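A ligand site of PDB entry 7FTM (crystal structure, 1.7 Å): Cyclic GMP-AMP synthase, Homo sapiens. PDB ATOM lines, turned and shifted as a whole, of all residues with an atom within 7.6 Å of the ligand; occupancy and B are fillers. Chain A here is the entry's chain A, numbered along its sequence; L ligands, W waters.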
ATOM      1  N   GLY A   1     -22.461 -15.709 -13.142  1.00  0.00           N
ATOM      2  CA  GLY A   1     -22.241 -16.896 -12.340  1.00  0.00           C
ATOM      3  C   GLY A   1     -21.029 -16.773 -11.448  1.00  0.00           C
ATOM      4  O   GLY A   1     -20.577 -15.662 -11.177  1.00  0.00           O
ATOM      5  N   ALA A   2     -20.490 -17.913 -11.003  1.00  0.00           N
ATOM      6  CA  ALA A   2     -19.278 -17.896 -10.185  1.00  0.00           C
ATOM      7  C   ALA A   2     -18.123 -17.191 -10.883  1.00  0.00           C
ATOM      8  O   ALA A   2     -17.185 -16.755 -10.210  1.00  0.00           O
ATOM      9  CB  ALA A   2     -18.850 -19.315  -9.826  1.00  0.00           C
ATOM     10  N   SER A   3     -18.163 -17.049 -12.217  1.00  0.00           N
ATOM     11  CA  SER A   3     -17.168 -16.206 -12.870  1.00  0.00           C
ATOM     12  C   SER A   3     -17.192 -14.796 -12.291  1.00  0.00           C
ATOM     13  O   SER A   3     -16.149 -14.155 -12.160  1.00  0.00           O
ATOM     14  CB  SER A   3     -17.383 -16.194 -14.385  1.00  0.00           C
ATOM     15  OG  SER A   3     -18.734 -15.856 -14.692  1.00  0.00           O
ATOM     16  N   LYS A   4     -18.376 -14.316 -11.894  1.00  0.00           N
ATOM     17  CA  LYS A   4     -18.443 -13.004 -11.257  1.00  0.00           C
ATOM     18  C   LYS A   4     -17.676 -12.986  -9.941  1.00  0.00           C
ATOM     19  O   LYS A   4     -17.048 -11.979  -9.597  1.00  0.00           O
ATOM     20  CB  LYS A   4     -19.909 -12.617 -11.027  1.00  0.00           C
ATOM     21  CG  LYS A   4     -20.132 -11.218 -10.479  1.00  0.00           C
ATOM     22  CD  LYS A   4     -21.608 -10.975 -10.105  1.00  0.00           C
ATOM     23  CE  LYS A   4     -22.553 -11.315 -11.246  1.00  0.00           C
ATOM     24  NZ  LYS A   4     -23.944 -10.832 -11.016  1.00  0.00           N
ATOM     25  N   LEU A   5     -17.756 -14.083  -9.171  1.00  0.00           N
ATOM     26  CA  LEU A   5     -17.034 -14.181  -7.905  1.00  0.00           C
ATOM     27  C   LEU A   5     -15.534 -14.324  -8.138  1.00  0.00           C
ATOM     28  O   LEU A   5     -14.721 -13.718  -7.435  1.00  0.00           O
ATOM     29  CB  LEU A   5     -17.535 -15.374  -7.097  1.00  0.00           C
ATOM     30  CG  LEU A   5     -19.006 -15.283  -6.652  1.00  0.00           C
ATOM     31  CD1 LEU A   5     -19.339 -16.549  -5.866  1.00  0.00           C
ATOM     32  CD2 LEU A   5     -19.239 -14.034  -5.796  1.00  0.00           C
ATOM     33  N   ARG A   6     -15.153 -15.161  -9.092  1.00  0.00           N
ATOM     34  CA  ARG A   6     -13.735 -15.321  -9.392  1.00  0.00           C
ATOM     35  C   ARG A   6     -13.158 -14.005  -9.893  1.00  0.00           C
ATOM     36  O   ARG A   6     -12.006 -13.674  -9.577  1.00  0.00           O
ATOM     37  CB  ARG A   6     -13.551 -16.466 -10.396  1.00  0.00           C
ATOM     38  CG  ARG A   6     -12.121 -16.958 -10.540  1.00  0.00           C
ATOM     39  CD  ARG A   6     -11.633 -17.670  -9.270  1.00  0.00           C
ATOM     40  NE  ARG A   6     -12.257 -18.975  -9.093  1.00  0.00           N
ATOM     41  CZ  ARG A   6     -12.119 -19.738  -8.008  1.00  0.00           C
ATOM     42  NH1 ARG A   6     -11.380 -19.320  -6.984  1.00  0.00           N
ATOM     43  NH2 ARG A   6     -12.720 -20.919  -7.946  1.00  0.00           N
ATOM     44  N   VAL A   8     -14.171 -10.981  -8.939  1.00  0.00           N
ATOM     45  CA  VAL A   8     -13.973 -10.150  -7.750  1.00  0.00           C
ATOM     46  C   VAL A   8     -12.666 -10.520  -7.043  1.00  0.00           C
ATOM     47  O   VAL A   8     -11.891  -9.642  -6.633  1.00  0.00           O
ATOM     48  CB  VAL A   8     -15.171 -10.293  -6.794  1.00  0.00           C
ATOM     49  CG1 VAL A   8     -14.801  -9.733  -5.433  1.00  0.00           C
ATOM     50  CG2 VAL A   8     -16.387  -9.599  -7.346  1.00  0.00           C
ATOM     51  N   LEU A 252     -14.838 -13.200   0.245  1.00  0.00           N
ATOM     52  CA  LEU A 252     -15.994 -12.663  -0.460  1.00  0.00           C
ATOM     53  C   LEU A 252     -17.074 -12.175   0.508  1.00  0.00           C
ATOM     54  O   LEU A 252     -17.749 -11.182   0.229  1.00  0.00           O
ATOM     55  CB  LEU A 252     -16.572 -13.715  -1.392  1.00  0.00           C
ATOM     56  CG  LEU A 252     -15.715 -14.016  -2.610  1.00  0.00           C
ATOM     57  CD1 LEU A 252     -16.239 -15.285  -3.319  1.00  0.00           C
ATOM     58  CD2 LEU A 252     -15.681 -12.811  -3.558  1.00  0.00           C
ATOM     59  N   LYS A 298     -14.229 -25.834  -7.471  1.00  0.00           N
ATOM     60  CA  LYS A 298     -15.169 -25.719  -8.582  1.00  0.00           C
ATOM     61  C   LYS A 298     -16.547 -25.274  -8.110  1.00  0.00           C
ATOM     62  O   LYS A 298     -17.346 -24.806  -8.942  1.00  0.00           O
ATOM     63  CB  LYS A 298     -15.312 -27.070  -9.307  1.00  0.00           C
ATOM     64  CG  LYS A 298     -14.038 -27.600  -9.927  1.00  0.00           C
ATOM     65  CD  LYS A 298     -14.333 -28.799 -10.823  1.00  0.00           C
ATOM     66  CE  LYS A 298     -15.107 -29.867 -10.059  1.00  0.00           C
ATOM     67  NZ  LYS A 298     -14.363 -30.341  -8.861  1.00  0.00           N
ATOM     68  N   ASP A 299     -16.846 -25.409  -6.826  1.00  0.00           N
ATOM     69  CA  ASP A 299     -18.159 -25.093  -6.284  1.00  0.00           C
ATOM     70  C   ASP A 299     -18.183 -23.759  -5.568  1.00  0.00           C
ATOM     71  O   ASP A 299     -19.005 -23.572  -4.660  1.00  0.00           O
ATOM     72  CB  ASP A 299     -18.631 -26.212  -5.351  1.00  0.00           C
ATOM     73  CG  ASP A 299     -18.833 -27.537  -6.077  1.00  0.00           C
ATOM     74  OD1 ASP A 299     -19.192 -27.505  -7.275  1.00  0.00           O
ATOM     75  OD2 ASP A 299     -18.629 -28.601  -5.456  1.00  0.00           O
ATOM     76  N   LEU A 300     -17.327 -22.807  -5.985  1.00  0.00           N
ATOM     77  CA  LEU A 300     -17.241 -21.517  -5.293  1.00  0.00           C
ATOM     78  C   LEU A 300     -18.608 -20.839  -5.152  1.00  0.00           C
ATOM     79  O   LEU A 300     -18.911 -20.257  -4.105  1.00  0.00           O
ATOM     80  CB  LEU A 300     -16.276 -20.580  -6.033  1.00  0.00           C
ATOM     81  CG  LEU A 300     -16.092 -19.191  -5.413  1.00  0.00           C
ATOM     82  CD1 LEU A 300     -15.447 -19.281  -4.044  1.00  0.00           C
ATOM     83  CD2 LEU A 300     -15.271 -18.283  -6.359  1.00  0.00           C
ATOM     84  N   GLY A 301     -19.426 -20.868  -6.211  1.00  0.00           N
ATOM     85  CA  GLY A 301     -20.704 -20.180  -6.163  1.00  0.00           C
ATOM     86  C   GLY A 301     -21.636 -20.778  -5.130  1.00  0.00           C
ATOM     87  O   GLY A 301     -22.228 -20.054  -4.314  1.00  0.00           O
ATOM     88  N   LEU A 302     -21.772 -22.107  -5.145  1.00  0.00           N
ATOM     89  CA  LEU A 302     -22.609 -22.804  -4.161  1.00  0.00           C
ATOM     90  C   LEU A 302     -22.117 -22.596  -2.736  1.00  0.00           C
ATOM     91  O   LEU A 302     -22.924 -22.421  -1.804  1.00  0.00           O
ATOM     92  CB  LEU A 302     -22.630 -24.291  -4.501  1.00  0.00           C
ATOM     93  CG  LEU A 302     -23.533 -25.202  -3.671  1.00  0.00           C
ATOM     94  CD1 LEU A 302     -24.984 -24.794  -3.867  1.00  0.00           C
ATOM     95  CD2 LEU A 302     -23.289 -26.639  -4.076  1.00  0.00           C
ATOM     96  N   CYS A 303     -20.796 -22.648  -2.533  1.00  0.00           N
ATOM     97  CA  CYS A 303     -20.230 -22.479  -1.204  1.00  0.00           C
ATOM     98  C   CYS A 303     -20.463 -21.065  -0.672  1.00  0.00           C
ATOM     99  O   CYS A 303     -20.877 -20.892   0.473  1.00  0.00           O
ATOM    100  CB  CYS A 303     -18.738 -22.809  -1.229  1.00  0.00           C
ATOM    101  SG  CYS A 303     -18.396 -24.545  -1.678  1.00  0.00           S
ATOM    102  N   PHE A 304     -20.251 -20.052  -1.512  1.00  0.00           N
ATOM    103  CA  PHE A 304     -20.568 -18.678  -1.113  1.00  0.00           C
ATOM    104  C   PHE A 304     -22.056 -18.539  -0.779  1.00  0.00           C
ATOM    105  O   PHE A 304     -22.423 -17.904   0.215  1.00  0.00           O
ATOM    106  CB  PHE A 304     -20.165 -17.704  -2.212  1.00  0.00           C
ATOM    107  CG  PHE A 304     -20.387 -16.257  -1.854  1.00  0.00           C
ATOM    108  CD1 PHE A 304     -19.704 -15.669  -0.809  1.00  0.00           C
ATOM    109  CD2 PHE A 304     -21.279 -15.476  -2.589  1.00  0.00           C
ATOM    110  CE1 PHE A 304     -19.895 -14.319  -0.485  1.00  0.00           C
ATOM    111  CE2 PHE A 304     -21.475 -14.130  -2.272  1.00  0.00           C
ATOM    112  CZ  PHE A 304     -20.779 -13.566  -1.221  1.00  0.00           C
ATOM    113  N   ASP A 305     -22.924 -19.148  -1.590  1.00  0.00           N
ATOM    114  CA  ASP A 305     -24.361 -19.142  -1.281  1.00  0.00           C
ATOM    115  C   ASP A 305     -24.650 -19.764   0.087  1.00  0.00           C
ATOM    116  O   ASP A 305     -25.498 -19.245   0.835  1.00  0.00           O
ATOM    117  CB  ASP A 305     -25.140 -19.849  -2.380  1.00  0.00           C
ATOM    118  CG  ASP A 305     -25.436 -18.948  -3.571  1.00  0.00           C
ATOM    119  OD1 ASP A 305     -25.540 -17.713  -3.389  1.00  0.00           O
ATOM    120  OD2 ASP A 305     -25.589 -19.475  -4.697  1.00  0.00           O
ATOM    121  N   VAL A 308     -23.715 -17.077   2.685  1.00  0.00           N
ATOM    122  CA  VAL A 308     -24.657 -15.959   2.721  1.00  0.00           C
ATOM    123  C   VAL A 308     -25.974 -16.393   3.335  1.00  0.00           C
ATOM    124  O   VAL A 308     -26.595 -15.646   4.104  1.00  0.00           O
ATOM    125  CB  VAL A 308     -24.865 -15.402   1.305  1.00  0.00           C
ATOM    126  CG1 VAL A 308     -26.020 -14.410   1.306  1.00  0.00           C
ATOM    127  CG2 VAL A 308     -23.592 -14.755   0.774  1.00  0.00           C
ATOM    128  N   GLU A 351     -29.527  -8.989  -2.631  1.00  0.00           N
ATOM    129  CA  GLU A 351     -28.306  -9.343  -3.357  1.00  0.00           C
ATOM    130  C   GLU A 351     -28.284 -10.823  -3.690  1.00  0.00           C
ATOM    131  O   GLU A 351     -28.009 -11.212  -4.830  1.00  0.00           O
ATOM    132  CB  GLU A 351     -27.064  -8.954  -2.545  1.00  0.00           C
ATOM    133  CG  GLU A 351     -26.895  -7.444  -2.414  1.00  0.00           C
ATOM    134  CD  GLU A 351     -26.564  -6.739  -3.726  1.00  0.00           C
ATOM    135  OE1 GLU A 351     -25.937  -7.377  -4.602  1.00  0.00           O
ATOM    136  OE2 GLU A 351     -26.905  -5.554  -3.875  1.00  0.00           O
ATOM    137  N   ARG A 352     -28.592 -11.675  -2.702  1.00  0.00           N
ATOM    138  CA  ARG A 352     -28.626 -13.116  -2.952  1.00  0.00           C
ATOM    139  C   ARG A 352     -29.654 -13.483  -4.020  1.00  0.00           C
ATOM    140  O   ARG A 352     -29.401 -14.341  -4.874  1.00  0.00           O
ATOM    141  CB  ARG A 352     -28.925 -13.864  -1.652  1.00  0.00           C
ATOM    142  CG  ARG A 352     -29.286 -15.312  -1.900  1.00  0.00           C
ATOM    143  CD  ARG A 352     -29.539 -16.112  -0.656  1.00  0.00           C
ATOM    144  NE  ARG A 352     -29.968 -17.457  -1.010  1.00  0.00           N
ATOM    145  CZ  ARG A 352     -29.135 -18.428  -1.379  1.00  0.00           C
ATOM    146  NH1 ARG A 352     -27.832 -18.197  -1.435  1.00  0.00           N
ATOM    147  NH2 ARG A 352     -29.616 -19.623  -1.704  1.00  0.00           N
ATOM    148  N   ASN A 354     -30.564 -11.842  -6.571  1.00  0.00           N
ATOM    149  CA  ASN A 354     -30.306 -11.291  -7.891  1.00  0.00           C
ATOM    150  C   ASN A 354     -28.854 -11.511  -8.328  1.00  0.00           C
ATOM    151  O   ASN A 354     -28.333 -10.757  -9.154  1.00  0.00           O
ATOM    152  CB  ASN A 354     -30.653  -9.810  -7.938  1.00  0.00           C
ATOM    153  CG  ASN A 354     -32.153  -9.583  -7.915  1.00  0.00           C
ATOM    154  OD1 ASN A 354     -32.758  -9.420  -6.847  1.00  0.00           O
ATOM    155  ND2 ASN A 354     -32.760  -9.566  -9.080  1.00  0.00           N
ATOM    156  N   GLU A 355     -28.201 -12.549  -7.793  1.00  0.00           N
ATOM    157  CA  GLU A 355     -26.845 -12.937  -8.215  1.00  0.00           C
ATOM    158  C   GLU A 355     -25.810 -11.865  -7.869  1.00  0.00           C
ATOM    159  O   GLU A 355     -24.852 -11.640  -8.625  1.00  0.00           O
ATOM    160  CB  GLU A 355     -26.792 -13.267  -9.706  1.00  0.00           C
ATOM    161  CG  GLU A 355     -27.462 -14.565 -10.095  1.00  0.00           C
ATOM    162  CD  GLU A 355     -26.534 -15.465 -10.882  1.00  0.00           C
ATOM    163  OE1 GLU A 355     -25.527 -15.934 -10.287  1.00  0.00           O
ATOM    164  OE2 GLU A 355     -26.786 -15.702 -12.079  1.00  0.00           O
ATOM    165  N   PHE A 356     -26.011 -11.196  -6.740  1.00  0.00           N
ATOM    166  CA  PHE A 356     -25.092 -10.208  -6.171  1.00  0.00           C
ATOM    167  C   PHE A 356     -24.709  -9.089  -7.151  1.00  0.00           C
ATOM    168  O   PHE A 356     -23.523  -8.979  -7.526  1.00  0.00           O
ATOM    169  CB  PHE A 356     -23.871 -10.928  -5.634  1.00  0.00           C
ATOM    170  CG  PHE A 356     -24.185 -11.820  -4.483  1.00  0.00           C
ATOM    171  CD1 PHE A 356     -24.215 -11.321  -3.200  1.00  0.00           C
ATOM    172  CD2 PHE A 356     -24.539 -13.145  -4.699  1.00  0.00           C
ATOM    173  CE1 PHE A 356     -24.534 -12.144  -2.126  1.00  0.00           C
ATOM    174  CE2 PHE A 356     -24.855 -13.976  -3.636  1.00  0.00           C
ATOM    175  CZ  PHE A 356     -24.855 -13.470  -2.351  1.00  0.00           C
ATOM    176  N   PRO A 357     -25.646  -8.232  -7.546  1.00  0.00           N
ATOM    177  CA  PRO A 357     -25.281  -7.142  -8.469  1.00  0.00           C
ATOM    178  C   PRO A 357     -24.314  -6.137  -7.861  1.00  0.00           C
ATOM    179  O   PRO A 357     -23.681  -5.383  -8.616  1.00  0.00           O
ATOM    180  CB  PRO A 357     -26.636  -6.491  -8.819  1.00  0.00           C
ATOM    181  CG  PRO A 357     -27.604  -6.982  -7.809  1.00  0.00           C
ATOM    182  CD  PRO A 357     -27.113  -8.320  -7.337  1.00  0.00           C
ATOM    183  N   PHE A 359     -21.569  -6.910  -6.939  1.00  0.00           N
ATOM    184  CA  PHE A 359     -20.294  -7.340  -7.510  1.00  0.00           C
ATOM    185  C   PHE A 359     -20.161  -7.071  -9.010  1.00  0.00           C
ATOM    186  O   PHE A 359     -19.145  -7.454  -9.604  1.00  0.00           O
ATOM    187  CB  PHE A 359     -20.097  -8.834  -7.243  1.00  0.00           C
ATOM    188  CG  PHE A 359     -19.844  -9.174  -5.794  1.00  0.00           C
ATOM    189  CD1 PHE A 359     -19.290  -8.241  -4.911  1.00  0.00           C
ATOM    190  CD2 PHE A 359     -20.136 -10.442  -5.304  1.00  0.00           C
ATOM    191  CE1 PHE A 359     -19.025  -8.580  -3.593  1.00  0.00           C
ATOM    192  CE2 PHE A 359     -19.865 -10.787  -3.959  1.00  0.00           C
ATOM    193  CZ  PHE A 359     -19.322  -9.852  -3.110  1.00  0.00           C
ATOM    194  N   ASP A 360     -21.138  -6.425  -9.648  1.00  0.00           N
ATOM    195  CA  ASP A 360     -21.107  -6.212 -11.086  1.00  0.00           C
ATOM    196  C   ASP A 360     -20.039  -5.183 -11.465  1.00  0.00           C
ATOM    197  O   ASP A 360     -19.662  -4.307 -10.683  1.00  0.00           O
ATOM    198  CB  ASP A 360     -22.463  -5.729 -11.608  1.00  0.00           C
ATOM    199  CG  ASP A 360     -23.487  -6.842 -11.682  1.00  0.00           C
ATOM    200  OD1 ASP A 360     -23.120  -8.014 -11.422  1.00  0.00           O
ATOM    201  OD2 ASP A 360     -24.658  -6.543 -11.997  1.00  0.00           O
HETATM  202  C1  LIG L   1     -23.284 -17.293  -7.222  1.00  0.00           C
HETATM  203  C2  LIG L   1     -22.376 -14.723  -7.624  1.00  0.00           C
HETATM  204  O1  LIG L   1     -23.088 -20.098 -11.858  1.00  0.00           O
HETATM  205  C3  LIG L   1     -23.238 -16.406  -6.162  1.00  0.00           C
HETATM  206  C4  LIG L   1     -22.778 -15.125  -6.358  1.00  0.00           C
HETATM  207  C5  LIG L   1     -22.420 -15.607  -8.714  1.00  0.00           C
HETATM  208  C6  LIG L   1     -23.729 -19.765  -7.723  1.00  0.00           C
HETATM  209  C7  LIG L   1     -22.875 -16.909  -8.509  1.00  0.00           C
HETATM  210  C8  LIG L   1     -23.162 -21.326  -9.238  1.00  0.00           C
HETATM  211  C9  LIG L   1     -22.406 -21.870 -10.407  1.00  0.00           C
HETATM  212  C10 LIG L   1     -24.091 -22.016  -8.531  1.00  0.00           C
HETATM  213  C11 LIG L   1     -22.033 -20.830 -11.428  1.00  0.00           C
HETATM  214  F1  LIG L   1     -21.940 -13.481  -7.795  1.00  0.00           F
HETATM  215  N1  LIG L   1     -22.912 -20.004  -8.787  1.00  0.00           N
HETATM  216  N2  LIG L   1     -23.775 -18.603  -6.973  1.00  0.00           N
HETATM  217  O2  LIG L   1     -20.922 -20.616 -11.893  1.00  0.00           O
HETATM  218  S1  LIG L   1     -24.756 -21.110  -7.257  1.00  0.00           S
HETATM  219  O   HOH W   1     -20.968 -23.268  -7.729  1.00  0.00           O
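N of Ala 2 is in hydrogen-bond range of O2 of the ligand, 2.9 Å away. The side-chain carboxylate (OD2) of Asp 305 sits at hydrogen-bond distance from a nitrogen (N2) of the ligand (3.0 Å). The backbone carbonyl oxygen of Gly 301 lies within hydrogen-bond range of a nitrogen (N2) of the ligand, at 3.4 Å. A sulfur (S1) of the ligand sits close to the backbone NH (N) of Leu 302 (3.8 Å).
The guanidinium group of Arg 352 is in salt-bridge range of the side-chain carboxylate of Asp 305. N of Phe 356 sits at hydrogen-bond distance from O of Glu 351. The backbone carbonyl oxygen (O) of Glu 355 is in hydrogen-bond range of the side-chain amino group (NZ) of Lys 4 (2.7 Å). The side-chain amino group (NZ) of Lys 4 is in salt-bridge range of the side-chain carboxylate (OD1) of Asp 360 (3.0 Å).
Gly 1 touches the ligand. Lys 4 touches the ligand (CD to F1, 3.4 Å). Leu 5 touches the ligand. Glu 355 touches the ligand. CD2 of Phe 356 touches C4 of the ligand (3.1 Å). Hydrophobic or aromatic side chains within 4 Å of the ligand: Ala 2, Leu 5 and Phe 356. Nine residues have an atom within 4 Å of the ligand: Gly 1, Ala 2, Lys 4, Leu 5, Gly 301, Leu 302, Asp 305, Glu 355 and Phe 356.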
